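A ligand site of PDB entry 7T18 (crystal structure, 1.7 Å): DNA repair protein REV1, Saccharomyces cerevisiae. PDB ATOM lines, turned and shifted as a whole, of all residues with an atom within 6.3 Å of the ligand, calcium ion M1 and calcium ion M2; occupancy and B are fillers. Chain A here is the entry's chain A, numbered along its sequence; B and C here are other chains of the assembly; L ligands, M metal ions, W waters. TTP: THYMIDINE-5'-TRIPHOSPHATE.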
ATOM      1  N   ARG A  29      20.862  15.791 -12.832  1.00  0.00           N
ATOM      2  CA  ARG A  29      22.005  14.902 -13.042  1.00  0.00           C
ATOM      3  C   ARG A  29      22.876  15.383 -14.195  1.00  0.00           C
ATOM      4  O   ARG A  29      24.109  15.297 -14.127  1.00  0.00           O
ATOM      5  CB  ARG A  29      21.537  13.467 -13.300  1.00  0.00           C
ATOM      6  CG  ARG A  29      20.875  13.249 -14.674  1.00  0.00           C
ATOM      7  CD  ARG A  29      20.175  11.919 -14.706  1.00  0.00           C
ATOM      8  NE  ARG A  29      20.116  11.334 -16.038  1.00  0.00           N
ATOM      9  CZ  ARG A  29      19.157  11.578 -16.923  1.00  0.00           C
ATOM     10  NH1 ARG A  29      18.190  12.428 -16.613  1.00  0.00           N
ATOM     11  NH2 ARG A  29      19.168  10.980 -18.111  1.00  0.00           N
ATOM     12  N   LEU A  30      22.260  15.896 -15.258  1.00  0.00           N
ATOM     13  CA  LEU A  30      23.043  16.285 -16.422  1.00  0.00           C
ATOM     14  C   LEU A  30      23.861  17.539 -16.132  1.00  0.00           C
ATOM     15  O   LEU A  30      24.986  17.684 -16.623  1.00  0.00           O
ATOM     16  CB  LEU A  30      22.142  16.451 -17.636  1.00  0.00           C
ATOM     17  CG  LEU A  30      21.511  15.134 -18.142  1.00  0.00           C
ATOM     18  CD1 LEU A  30      20.447  15.391 -19.197  1.00  0.00           C
ATOM     19  CD2 LEU A  30      22.567  14.231 -18.686  1.00  0.00           C
ATOM     20  N   LEU A  33      26.812  16.181 -14.247  1.00  0.00           N
ATOM     21  CA  LEU A  33      27.697  15.469 -15.214  1.00  0.00           C
ATOM     22  C   LEU A  33      28.647  16.469 -15.887  1.00  0.00           C
ATOM     23  O   LEU A  33      29.855  16.195 -15.935  1.00  0.00           O
ATOM     24  CB  LEU A  33      26.830  14.751 -16.248  1.00  0.00           C
ATOM     25  CG  LEU A  33      27.071  13.252 -16.386  1.00  0.00           C
ATOM     26  CD1 LEU A  33      26.641  12.752 -17.762  1.00  0.00           C
ATOM     27  CD2 LEU A  33      28.544  12.912 -16.140  1.00  0.00           C
ATOM     28  N   TRP A  36      30.978  18.417 -13.072  1.00  0.00           N
ATOM     29  CA  TRP A  36      32.051  17.532 -12.658  1.00  0.00           C
ATOM     30  C   TRP A  36      33.147  17.436 -13.706  1.00  0.00           C
ATOM     31  O   TRP A  36      34.334  17.494 -13.383  1.00  0.00           O
ATOM     32  CB  TRP A  36      31.495  16.138 -12.397  1.00  0.00           C
ATOM     33  CG  TRP A  36      30.655  16.018 -11.201  1.00  0.00           C
ATOM     34  CD1 TRP A  36      30.770  16.697 -10.025  1.00  0.00           C
ATOM     35  CD2 TRP A  36      29.556  15.119 -11.038  1.00  0.00           C
ATOM     36  NE1 TRP A  36      29.803  16.276  -9.141  1.00  0.00           N
ATOM     37  CE2 TRP A  36      29.052  15.299  -9.746  1.00  0.00           C
ATOM     38  CE3 TRP A  36      28.964  14.149 -11.869  1.00  0.00           C
ATOM     39  CZ2 TRP A  36      27.972  14.565  -9.259  1.00  0.00           C
ATOM     40  CZ3 TRP A  36      27.902  13.427 -11.388  1.00  0.00           C
ATOM     41  CH2 TRP A  36      27.412  13.645 -10.097  1.00  0.00           C
ATOM     42  N   ASP A  67      36.252   2.351 -15.805  1.00  0.00           N
ATOM     43  CA  ASP A  67      34.939   2.972 -15.674  1.00  0.00           C
ATOM     44  C   ASP A  67      34.131   2.239 -14.603  1.00  0.00           C
ATOM     45  O   ASP A  67      34.130   1.003 -14.564  1.00  0.00           O
ATOM     46  CB  ASP A  67      34.214   2.952 -17.035  1.00  0.00           C
ATOM     47  CG  ASP A  67      32.754   3.350 -16.937  1.00  0.00           C
ATOM     48  OD1 ASP A  67      31.914   2.461 -16.750  1.00  0.00           O
ATOM     49  OD2 ASP A  67      32.462   4.555 -17.035  1.00  0.00           O
ATOM     50  N   PHE A  68      33.469   2.995 -13.721  1.00  0.00           N
ATOM     51  CA  PHE A  68      32.601   2.393 -12.705  1.00  0.00           C
ATOM     52  C   PHE A  68      31.419   1.674 -13.363  1.00  0.00           C
ATOM     53  O   PHE A  68      30.755   2.228 -14.245  1.00  0.00           O
ATOM     54  CB  PHE A  68      32.001   3.473 -11.790  1.00  0.00           C
ATOM     55  CG  PHE A  68      32.898   3.996 -10.695  1.00  0.00           C
ATOM     56  CD1 PHE A  68      33.920   4.880 -10.971  1.00  0.00           C
ATOM     57  CD2 PHE A  68      32.621   3.699  -9.371  1.00  0.00           C
ATOM     58  CE1 PHE A  68      34.703   5.435  -9.954  1.00  0.00           C
ATOM     59  CE2 PHE A  68      33.381   4.246  -8.336  1.00  0.00           C
ATOM     60  CZ  PHE A  68      34.428   5.100  -8.624  1.00  0.00           C
ATOM     61  N   ASP A  69      31.112   0.491 -12.869  1.00  0.00           N
ATOM     62  CA  ASP A  69      29.879  -0.197 -13.288  1.00  0.00           C
ATOM     63  C   ASP A  69      28.687   0.510 -12.627  1.00  0.00           C
ATOM     64  O   ASP A  69      28.738   0.700 -11.451  1.00  0.00           O
ATOM     65  CB  ASP A  69      29.881  -1.665 -12.833  1.00  0.00           C
ATOM     66  CG  ASP A  69      31.101  -2.402 -13.343  1.00  0.00           C
ATOM     67  OD1 ASP A  69      31.390  -2.248 -14.498  1.00  0.00           O
ATOM     68  OD2 ASP A  69      31.718  -3.060 -12.573  1.00  0.00           O
ATOM     69  N   CYS A  70      27.623   0.687 -13.389  1.00  0.00           N
ATOM     70  CA  CYS A  70      26.366   1.387 -13.034  1.00  0.00           C
ATOM     71  C   CYS A  70      26.609   2.402 -11.916  1.00  0.00           C
ATOM     72  O   CYS A  70      26.105   2.225 -10.868  1.00  0.00           O
ATOM     73  CB  CYS A  70      25.247   0.407 -12.718  1.00  0.00           C
ATOM     74  SG  CYS A  70      25.731  -0.907 -11.563  1.00  0.00           S
ATOM     75  N   PHE A  71      27.404   3.431 -12.235  1.00  0.00           N
ATOM     76  CA  PHE A  71      27.917   4.299 -11.184  1.00  0.00           C
ATOM     77  C   PHE A  71      26.882   4.813 -10.181  1.00  0.00           C
ATOM     78  O   PHE A  71      26.994   4.572  -8.980  1.00  0.00           O
ATOM     79  CB  PHE A  71      28.635   5.470 -11.849  1.00  0.00           C
ATOM     80  CG  PHE A  71      29.282   6.414 -10.898  1.00  0.00           C
ATOM     81  CD1 PHE A  71      30.124   5.951  -9.914  1.00  0.00           C
ATOM     82  CD2 PHE A  71      29.027   7.783 -10.986  1.00  0.00           C
ATOM     83  CE1 PHE A  71      30.733   6.821  -9.036  1.00  0.00           C
ATOM     84  CE2 PHE A  71      29.619   8.662 -10.094  1.00  0.00           C
ATOM     85  CZ  PHE A  71      30.476   8.184  -9.130  1.00  0.00           C
ATOM     86  N   PHE A  72      25.864   5.557 -10.647  1.00  0.00           N
ATOM     87  CA  PHE A  72      24.908   6.121  -9.691  1.00  0.00           C
ATOM     88  C   PHE A  72      24.177   5.020  -8.937  1.00  0.00           C
ATOM     89  O   PHE A  72      23.878   5.178  -7.744  1.00  0.00           O
ATOM     90  CB  PHE A  72      23.876   7.002 -10.379  1.00  0.00           C
ATOM     91  CG  PHE A  72      24.347   8.382 -10.764  1.00  0.00           C
ATOM     92  CD1 PHE A  72      25.685   8.739 -10.807  1.00  0.00           C
ATOM     93  CD2 PHE A  72      23.387   9.340 -11.113  1.00  0.00           C
ATOM     94  CE1 PHE A  72      26.066  10.018 -11.193  1.00  0.00           C
ATOM     95  CE2 PHE A  72      23.758  10.630 -11.491  1.00  0.00           C
ATOM     96  CZ  PHE A  72      25.105  10.955 -11.551  1.00  0.00           C
ATOM     97  N   ALA A  73      23.821   3.923  -9.611  1.00  0.00           N
ATOM     98  CA  ALA A  73      23.087   2.859  -8.910  1.00  0.00           C
ATOM     99  C   ALA A  73      23.955   2.218  -7.833  1.00  0.00           C
ATOM    100  O   ALA A  73      23.480   1.970  -6.728  1.00  0.00           O
ATOM    101  CB  ALA A  73      22.585   1.808  -9.903  1.00  0.00           C
ATOM    102  N   ALA A 106      18.522   7.407 -14.187  1.00  0.00           N
ATOM    103  CA  ALA A 106      19.902   7.874 -14.316  1.00  0.00           C
ATOM    104  C   ALA A 106      20.866   6.708 -14.441  1.00  0.00           C
ATOM    105  O   ALA A 106      21.836   6.775 -15.210  1.00  0.00           O
ATOM    106  CB  ALA A 106      20.253   8.755 -13.118  1.00  0.00           C
ATOM    107  N   SER A 107      20.619   5.642 -13.687  1.00  0.00           N
ATOM    108  CA  SER A 107      21.459   4.455 -13.680  1.00  0.00           C
ATOM    109  C   SER A 107      20.600   3.298 -13.228  1.00  0.00           C
ATOM    110  O   SER A 107      19.716   3.458 -12.384  1.00  0.00           O
ATOM    111  CB  SER A 107      22.651   4.637 -12.726  1.00  0.00           C
ATOM    112  OG  SER A 107      23.585   3.563 -12.822  1.00  0.00           O
ATOM    113  N   CYS A 108      20.857   2.132 -13.802  1.00  0.00           N
ATOM    114  CA  CYS A 108      20.190   0.930 -13.329  1.00  0.00           C
ATOM    115  C   CYS A 108      21.250  -0.151 -13.179  1.00  0.00           C
ATOM    116  O   CYS A 108      22.236  -0.161 -13.910  1.00  0.00           O
ATOM    117  CB  CYS A 108      19.093   0.467 -14.289  1.00  0.00           C
ATOM    118  SG  CYS A 108      19.677   0.239 -15.984  1.00  0.00           S
ATOM    119  N   TYR A 110      22.734  -4.174 -12.984  1.00  0.00           N
ATOM    120  CA  TYR A 110      22.751  -5.163 -14.052  1.00  0.00           C
ATOM    121  C   TYR A 110      21.641  -6.192 -13.903  1.00  0.00           C
ATOM    122  O   TYR A 110      21.290  -6.848 -14.889  1.00  0.00           O
ATOM    123  CB  TYR A 110      24.155  -5.807 -14.130  1.00  0.00           C
ATOM    124  CG  TYR A 110      25.094  -4.901 -14.899  1.00  0.00           C
ATOM    125  CD1 TYR A 110      25.614  -3.755 -14.316  1.00  0.00           C
ATOM    126  CD2 TYR A 110      25.428  -5.163 -16.218  1.00  0.00           C
ATOM    127  CE1 TYR A 110      26.448  -2.890 -15.034  1.00  0.00           C
ATOM    128  CE2 TYR A 110      26.277  -4.317 -16.940  1.00  0.00           C
ATOM    129  CZ  TYR A 110      26.771  -3.183 -16.345  1.00  0.00           C
ATOM    130  OH  TYR A 110      27.595  -2.331 -17.046  1.00  0.00           O
ATOM    131  N   ARG A 113      19.087  -4.510 -15.898  1.00  0.00           N
ATOM    132  CA  ARG A 113      19.444  -4.607 -17.304  1.00  0.00           C
ATOM    133  C   ARG A 113      19.177  -5.983 -17.878  1.00  0.00           C
ATOM    134  O   ARG A 113      18.983  -6.109 -19.089  1.00  0.00           O
ATOM    135  CB  ARG A 113      20.919  -4.231 -17.498  1.00  0.00           C
ATOM    136  CG  ARG A 113      21.221  -2.777 -17.127  1.00  0.00           C
ATOM    137  CD  ARG A 113      22.695  -2.413 -17.293  1.00  0.00           C
ATOM    138  NE  ARG A 113      22.976  -1.147 -16.615  1.00  0.00           N
ATOM    139  CZ  ARG A 113      23.986  -0.336 -16.901  1.00  0.00           C
ATOM    140  NH1 ARG A 113      24.839  -0.653 -17.872  1.00  0.00           N
ATOM    141  NH2 ARG A 113      24.137   0.798 -16.219  1.00  0.00           N
ATOM    142  N   ASN A 119      19.774   2.703 -18.939  1.00  0.00           N
ATOM    143  CA  ASN A 119      19.908   4.092 -18.520  1.00  0.00           C
ATOM    144  C   ASN A 119      19.157   4.988 -19.492  1.00  0.00           C
ATOM    145  O   ASN A 119      19.203   4.794 -20.714  1.00  0.00           O
ATOM    146  CB  ASN A 119      21.381   4.516 -18.489  1.00  0.00           C
ATOM    147  CG  ASN A 119      22.160   3.879 -17.356  1.00  0.00           C
ATOM    148  OD1 ASN A 119      21.623   3.098 -16.588  1.00  0.00           O
ATOM    149  ND2 ASN A 119      23.448   4.225 -17.254  1.00  0.00           N
ATOM    150  N   TYR A 141      18.888  10.059  -5.682  1.00  0.00           N
ATOM    151  CA  TYR A 141      20.241  10.508  -5.946  1.00  0.00           C
ATOM    152  C   TYR A 141      20.985  10.841  -4.656  1.00  0.00           C
ATOM    153  O   TYR A 141      20.412  11.318  -3.674  1.00  0.00           O
ATOM    154  CB  TYR A 141      20.224  11.755  -6.822  1.00  0.00           C
ATOM    155  CG  TYR A 141      19.661  11.583  -8.204  1.00  0.00           C
ATOM    156  CD1 TYR A 141      18.291  11.699  -8.442  1.00  0.00           C
ATOM    157  CD2 TYR A 141      20.490  11.334  -9.292  1.00  0.00           C
ATOM    158  CE1 TYR A 141      17.766  11.566  -9.716  1.00  0.00           C
ATOM    159  CE2 TYR A 141      19.973  11.203 -10.572  1.00  0.00           C
ATOM    160  CZ  TYR A 141      18.622  11.338 -10.779  1.00  0.00           C
ATOM    161  OH  TYR A 141      18.120  11.212 -12.072  1.00  0.00           O
ATOM    162  N   ILE A 169      37.886  11.386 -18.061  1.00  0.00           N
ATOM    163  CA  ILE A 169      36.822  11.361 -19.043  1.00  0.00           C
ATOM    164  C   ILE A 169      35.513  11.856 -18.440  1.00  0.00           C
ATOM    165  O   ILE A 169      34.783  12.623 -19.064  1.00  0.00           O
ATOM    166  CB  ILE A 169      36.645   9.942 -19.621  1.00  0.00           C
ATOM    167  CG1 ILE A 169      37.928   9.469 -20.294  1.00  0.00           C
ATOM    168  CG2 ILE A 169      35.470   9.896 -20.584  1.00  0.00           C
ATOM    169  CD1 ILE A 169      38.294  10.289 -21.527  1.00  0.00           C
ATOM    170  N   SER A 170      35.225  11.421 -17.213  1.00  0.00           N
ATOM    171  CA  SER A 170      33.999  11.824 -16.544  1.00  0.00           C
ATOM    172  C   SER A 170      34.152  11.532 -15.054  1.00  0.00           C
ATOM    173  O   SER A 170      35.218  11.109 -14.590  1.00  0.00           O
ATOM    174  CB  SER A 170      32.793  11.088 -17.125  1.00  0.00           C
ATOM    175  OG  SER A 170      32.663   9.840 -16.506  1.00  0.00           O
ATOM    176  N   ILE A 171      33.085  11.795 -14.311  1.00  0.00           N
ATOM    177  CA  ILE A 171      33.046  11.560 -12.871  1.00  0.00           C
ATOM    178  C   ILE A 171      33.458  10.123 -12.539  1.00  0.00           C
ATOM    179  O   ILE A 171      34.081   9.869 -11.500  1.00  0.00           O
ATOM    180  CB  ILE A 171      31.632  11.898 -12.341  1.00  0.00           C
ATOM    181  CG1 ILE A 171      31.579  11.776 -10.811  1.00  0.00           C
ATOM    182  CG2 ILE A 171      30.555  10.996 -12.973  1.00  0.00           C
ATOM    183  CD1 ILE A 171      32.178  12.967 -10.116  1.00  0.00           C
ATOM    184  N   ASP A 172      33.137   9.170 -13.422  1.00  0.00           N
ATOM    185  CA  ASP A 172      33.356   7.757 -13.121  1.00  0.00           C
ATOM    186  C   ASP A 172      34.249   7.049 -14.141  1.00  0.00           C
ATOM    187  O   ASP A 172      34.232   5.816 -14.217  1.00  0.00           O
ATOM    188  CB  ASP A 172      32.011   7.015 -13.003  1.00  0.00           C
ATOM    189  CG  ASP A 172      31.426   6.646 -14.356  1.00  0.00           C
ATOM    190  OD1 ASP A 172      31.599   7.421 -15.307  1.00  0.00           O
ATOM    191  OD2 ASP A 172      30.800   5.576 -14.477  1.00  0.00           O
ATOM    192  N   GLU A 173      35.052   7.786 -14.912  1.00  0.00           N
ATOM    193  CA  GLU A 173      35.719   7.146 -16.034  1.00  0.00           C
ATOM    194  C   GLU A 173      37.015   7.877 -16.343  1.00  0.00           C
ATOM    195  O   GLU A 173      37.028   9.110 -16.401  1.00  0.00           O
ATOM    196  CB  GLU A 173      34.805   7.137 -17.263  1.00  0.00           C
ATOM    197  CG  GLU A 173      35.366   6.452 -18.482  1.00  0.00           C
ATOM    198  CD  GLU A 173      34.364   6.480 -19.626  1.00  0.00           C
ATOM    199  OE1 GLU A 173      34.733   6.137 -20.773  1.00  0.00           O
ATOM    200  OE2 GLU A 173      33.201   6.848 -19.362  1.00  0.00           O
ATOM    201  N   LYS A 230      32.384  -5.544 -19.102  1.00  0.00           N
ATOM    202  CA  LYS A 230      31.364  -5.260 -18.102  1.00  0.00           C
ATOM    203  C   LYS A 230      30.412  -6.437 -17.914  1.00  0.00           C
ATOM    204  O   LYS A 230      30.141  -7.180 -18.869  1.00  0.00           O
ATOM    205  CB  LYS A 230      30.558  -4.019 -18.514  1.00  0.00           C
ATOM    206  CG  LYS A 230      31.310  -2.717 -18.269  1.00  0.00           C
ATOM    207  CD  LYS A 230      30.556  -1.513 -18.793  1.00  0.00           C
ATOM    208  CE  LYS A 230      31.122  -0.223 -18.197  1.00  0.00           C
ATOM    209  NZ  LYS A 230      31.134  -0.222 -16.689  1.00  0.00           N
ATOM    210  P    DG B  12      33.181  10.002 -24.016  1.00  0.00           P
ATOM    211  OP1  DG B  12      34.587  10.514 -24.129  1.00  0.00           O
ATOM    212  OP2  DG B  12      32.900   8.621 -24.320  1.00  0.00           O
ATOM    213  O5'  DG B  12      32.713  10.241 -22.530  1.00  0.00           O
ATOM    214  C5'  DG B  12      31.916   9.310 -21.808  1.00  0.00           C
ATOM    215  C4'  DG B  12      31.222  10.108 -20.740  1.00  0.00           C
ATOM    216  O4'  DG B  12      30.539  11.176 -21.422  1.00  0.00           O
ATOM    217  C3'  DG B  12      30.159   9.405 -19.916  1.00  0.00           C
ATOM    218  O3'  DG B  12      30.709   8.845 -18.724  1.00  0.00           O
ATOM    219  C2'  DG B  12      29.236  10.545 -19.559  1.00  0.00           C
ATOM    220  C1'  DG B  12      29.491  11.604 -20.643  1.00  0.00           C
ATOM    221  N9   DG B  12      28.328  11.816 -21.495  1.00  0.00           N
ATOM    222  C8   DG B  12      27.562  10.882 -22.151  1.00  0.00           C
ATOM    223  N7   DG B  12      26.473  11.379 -22.649  1.00  0.00           N
ATOM    224  C5   DG B  12      26.475  12.694 -22.224  1.00  0.00           C
ATOM    225  C6   DG B  12      25.525  13.722 -22.422  1.00  0.00           C
ATOM    226  O6   DG B  12      24.489  13.694 -23.066  1.00  0.00           O
ATOM    227  N1   DG B  12      25.936  14.923 -21.837  1.00  0.00           N
ATOM    228  C2   DG B  12      27.077  15.076 -21.100  1.00  0.00           C
ATOM    229  N2   DG B  12      27.281  16.275 -20.572  1.00  0.00           N
ATOM    230  N3   DG B  12      27.964  14.125 -20.901  1.00  0.00           N
ATOM    231  C4   DG B  12      27.621  12.976 -21.514  1.00  0.00           C
ATOM    232  P    DC C   5      18.551  20.532 -20.068  1.00  0.00           P
ATOM    233  OP1  DC C   5      17.590  21.356 -19.311  1.00  0.00           O
ATOM    234  OP2  DC C   5      18.693  20.743 -21.523  1.00  0.00           O
ATOM    235  O5'  DC C   5      20.026  20.665 -19.485  1.00  0.00           O
ATOM    236  C5'  DC C   5      20.247  20.539 -18.093  1.00  0.00           C
ATOM    237  C4'  DC C   5      21.724  20.557 -17.774  1.00  0.00           C
ATOM    238  O4'  DC C   5      22.361  19.372 -18.299  1.00  0.00           O
ATOM    239  C3'  DC C   5      22.501  21.719 -18.370  1.00  0.00           C
ATOM    240  O3'  DC C   5      23.560  22.010 -17.504  1.00  0.00           O
ATOM    241  C2'  DC C   5      23.012  21.154 -19.700  1.00  0.00           C
ATOM    242  C1'  DC C   5      23.291  19.709 -19.322  1.00  0.00           C
ATOM    243  N1   DC C   5      23.092  18.717 -20.411  1.00  0.00           N
ATOM    244  C2   DC C   5      24.135  17.865 -20.757  1.00  0.00           C
ATOM    245  O2   DC C   5      25.228  17.995 -20.184  1.00  0.00           O
ATOM    246  N3   DC C   5      23.923  16.916 -21.686  1.00  0.00           N
ATOM    247  C4   DC C   5      22.739  16.808 -22.264  1.00  0.00           C
ATOM    248  N4   DC C   5      22.576  15.865 -23.179  1.00  0.00           N
ATOM    249  C5   DC C   5      21.641  17.659 -21.918  1.00  0.00           C
ATOM    250  C6   DC C   5      21.867  18.580 -20.984  1.00  0.00           C
HETATM  251  PA  TTP L   1      27.755   5.788 -17.638  1.00  0.00           P
HETATM  252  O1A TTP L   1      29.126   5.350 -17.423  1.00  0.00           O
HETATM  253  O2A TTP L   1      27.374   5.997 -19.031  1.00  0.00           O
HETATM  254  O3A TTP L   1      26.728   4.718 -17.051  1.00  0.00           O
HETATM  255  PB  TTP L   1      26.714   3.727 -15.798  1.00  0.00           P
HETATM  256  O1B TTP L   1      27.982   3.861 -15.123  1.00  0.00           O
HETATM  257  O2B TTP L   1      25.435   3.976 -14.960  1.00  0.00           O
HETATM  258  O3B TTP L   1      26.607   2.269 -16.417  1.00  0.00           O
HETATM  259  PG  TTP L   1      27.727   1.385 -17.135  1.00  0.00           P
HETATM  260  O1G TTP L   1      28.933   2.263 -17.288  1.00  0.00           O
HETATM  261  O2G TTP L   1      28.023   0.164 -16.235  1.00  0.00           O
HETATM  262  O3G TTP L   1      27.118   0.922 -18.471  1.00  0.00           O
HETATM  263  O5' TTP L   1      27.486   7.115 -16.827  1.00  0.00           O
HETATM  264  C5' TTP L   1      28.008   7.328 -15.511  1.00  0.00           C
HETATM  265  C4' TTP L   1      26.950   7.965 -14.651  1.00  0.00           C
HETATM  266  O4' TTP L   1      26.661   9.262 -15.192  1.00  0.00           O
HETATM  267  C3' TTP L   1      25.618   7.223 -14.646  1.00  0.00           C
HETATM  268  O3' TTP L   1      25.550   6.271 -13.586  1.00  0.00           O
HETATM  269  C2' TTP L   1      24.597   8.322 -14.485  1.00  0.00           C
HETATM  270  C1' TTP L   1      25.268   9.536 -15.109  1.00  0.00           C
HETATM  271  N1  TTP L   1      24.777   9.822 -16.461  1.00  0.00           N
HETATM  272  C2  TTP L   1      23.645  10.633 -16.588  1.00  0.00           C
HETATM  273  O2  TTP L   1      23.102  11.084 -15.595  1.00  0.00           O
HETATM  274  N3  TTP L   1      23.154  10.926 -17.857  1.00  0.00           N
HETATM  275  C4  TTP L   1      23.792  10.350 -18.878  1.00  0.00           C
HETATM  276  O4  TTP L   1      23.327  10.605 -19.985  1.00  0.00           O
HETATM  277  C5  TTP L   1      24.927   9.515 -18.820  1.00  0.00           C
HETATM  278  C5M TTP L   1      25.590   8.927 -20.040  1.00  0.00           C
HETATM  279  C6  TTP L   1      25.436   9.190 -17.558  1.00  0.00           C
HETATM  280 CA    CA M   1      30.184   3.791 -15.910  1.00  0.00          CA
HETATM  281 CA    CA M   2      31.294   6.720 -17.620  1.00  0.00          CA
HETATM  282  O   HOH W   1      28.275  -0.065 -20.740  1.00  0.00           O
HETATM  283  O   HOH W   2      21.311   8.091 -20.301  1.00  0.00           O
HETATM  284  O   HOH W   3      21.456   8.843 -16.925  1.00  0.00           O
HETATM  285  O   HOH W   4      22.501  11.799 -22.735  1.00  0.00           O
HETATM  286  O   HOH W   5      24.729   5.556 -19.480  1.00  0.00           O
HETATM  287  O   HOH W   6      25.196   2.404 -19.942  1.00  0.00           O
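Water W5 bridges O2A of the ligand (2.7 Å) and ND2 of Asn 119 (2.9 Å).
Water W3 lies within hydrogen-bond range of the backbone carbonyl oxygen of Ala 106 (2.7 Å), a nitrogen (N3) of the ligand (2.8 Å) and the guanidinium group of Arg 29 (3.0 Å).
Water W4 lies within hydrogen-bond range of O6 of DG 12 of chain B and an oxygen (O4) of the ligand.
Merely in contact with calcium ion M2: Ser 170.
Of the 26 residues printed, 5 come within 4 Å of calcium ion M2.
The nearest printed residue that does not touch calcium ion M2 is Phe 68 (5.6 Å).
The side-chain amino group of Lys 230 is in salt-bridge range of an oxygen (O2G) of the ligand (3.2 Å).
The backbone NH of Phe 71 sits at hydrogen-bond distance from an oxygen (O2B) of the ligand (3.4 Å).
ND2 of Asn 119 sits at hydrogen-bond distance from O2B of the ligand (3.0 Å).
NE of Arg 29 lies within hydrogen-bond range of O2 of the ligand, at 3.0 Å.
The side-chain hydroxyl (OH) of Tyr 110 sits at hydrogen-bond distance from an oxygen (O2G) of the ligand (2.7 Å).
The backbone NH of Cys 70 sits at hydrogen-bond distance from an oxygen (O2G) of the ligand (2.9 Å).
The guanidinium group (NH1) of Arg 113 is in salt-bridge range of an oxygen (O3G) of the ligand (2.8 Å).
An oxygen (O3') of the ligand is in hydrogen-bond range of the backbone NH of Phe 72, 3.0 Å away.
O2B of the ligand sits at hydrogen-bond distance from OG of Ser 107 (2.9 Å).
Of the 26 residues printed, 3 come within 4 Å of calcium ion M1.
Along chain A the residues within 4 Å of calcium ion M1 span positions 67 to 172.
The nearest printed residue that does not touch calcium ion M1 is Lys 230 (4.2 Å).
Calcium ion M1 is bound by the side-chain carboxylate (OD1) of Asp 67 (2.3 Å), an oxygen (O1B) of the ligand (2.3 Å), the backbone carbonyl oxygen (O) of Phe 68 (2.4 Å), the side-chain carboxylate (OD2) of Asp 172 (2.4 Å), an oxygen (O1G) of the ligand (2.4 Å), an oxygen (O1A) of the ligand (2.4 Å) and the side-chain carboxylate (OD2) of Asp 67 (2.7 Å).
Merely in contact with the ligand: Leu 30, Leu 33, Asp 69 and Ala 106.
17 residues have an atom within 4 Å of the ligand: Arg 29, Leu 30, Leu 33, Asp 67, Phe 68, Asp 69, Cys 70, Phe 71, Phe 72, Ala 106, Ser 107, Tyr 110, Arg 113, Asn 119, Asp 172, Lys 230 and DG 12 of chain B.
Calcium ion M2 is bound by OD1 of Asp 172 (2.4 Å), O3' of DG 12 of chain B (2.5 Å), OD2 of Asp 67 (2.5 Å), O1A of the ligand (2.6 Å) and OE2 of Glu 173 (2.6 Å).
Calcium ion M2 has five donor atoms within binding distance.
The side-chain carboxylate (OD1) of Asp 67 sits close to the side-chain amino group (NZ) of Lys 230 (2.8 Å).
N2 of DG 12 of chain B lies close to O2 of DC 5 of chain C (2.7 Å).
The side-chain amino group (NZ) of Lys 230 lies within salt-bridge range of the side-chain carboxylate (OD1) of Asp 69 (3.0 Å).
NZ of Lys 230 sits close to O of Phe 68 (3.5 Å).
The backbone NH (N) of Asp 172 lies close to the side-chain hydroxyl (OG) of Ser 170, at 3.2 Å.
OD1 of Asn 119 is in hydrogen-bond range of NH2 of Arg 113, 3.4 Å away.
OG of Ser 107 lies close to O of Cys 70 (3.5 Å).
The side-chain hydroxyl of Tyr 110 sits at hydrogen-bond distance from the guanidinium group of Arg 113, at 3.3 Å.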
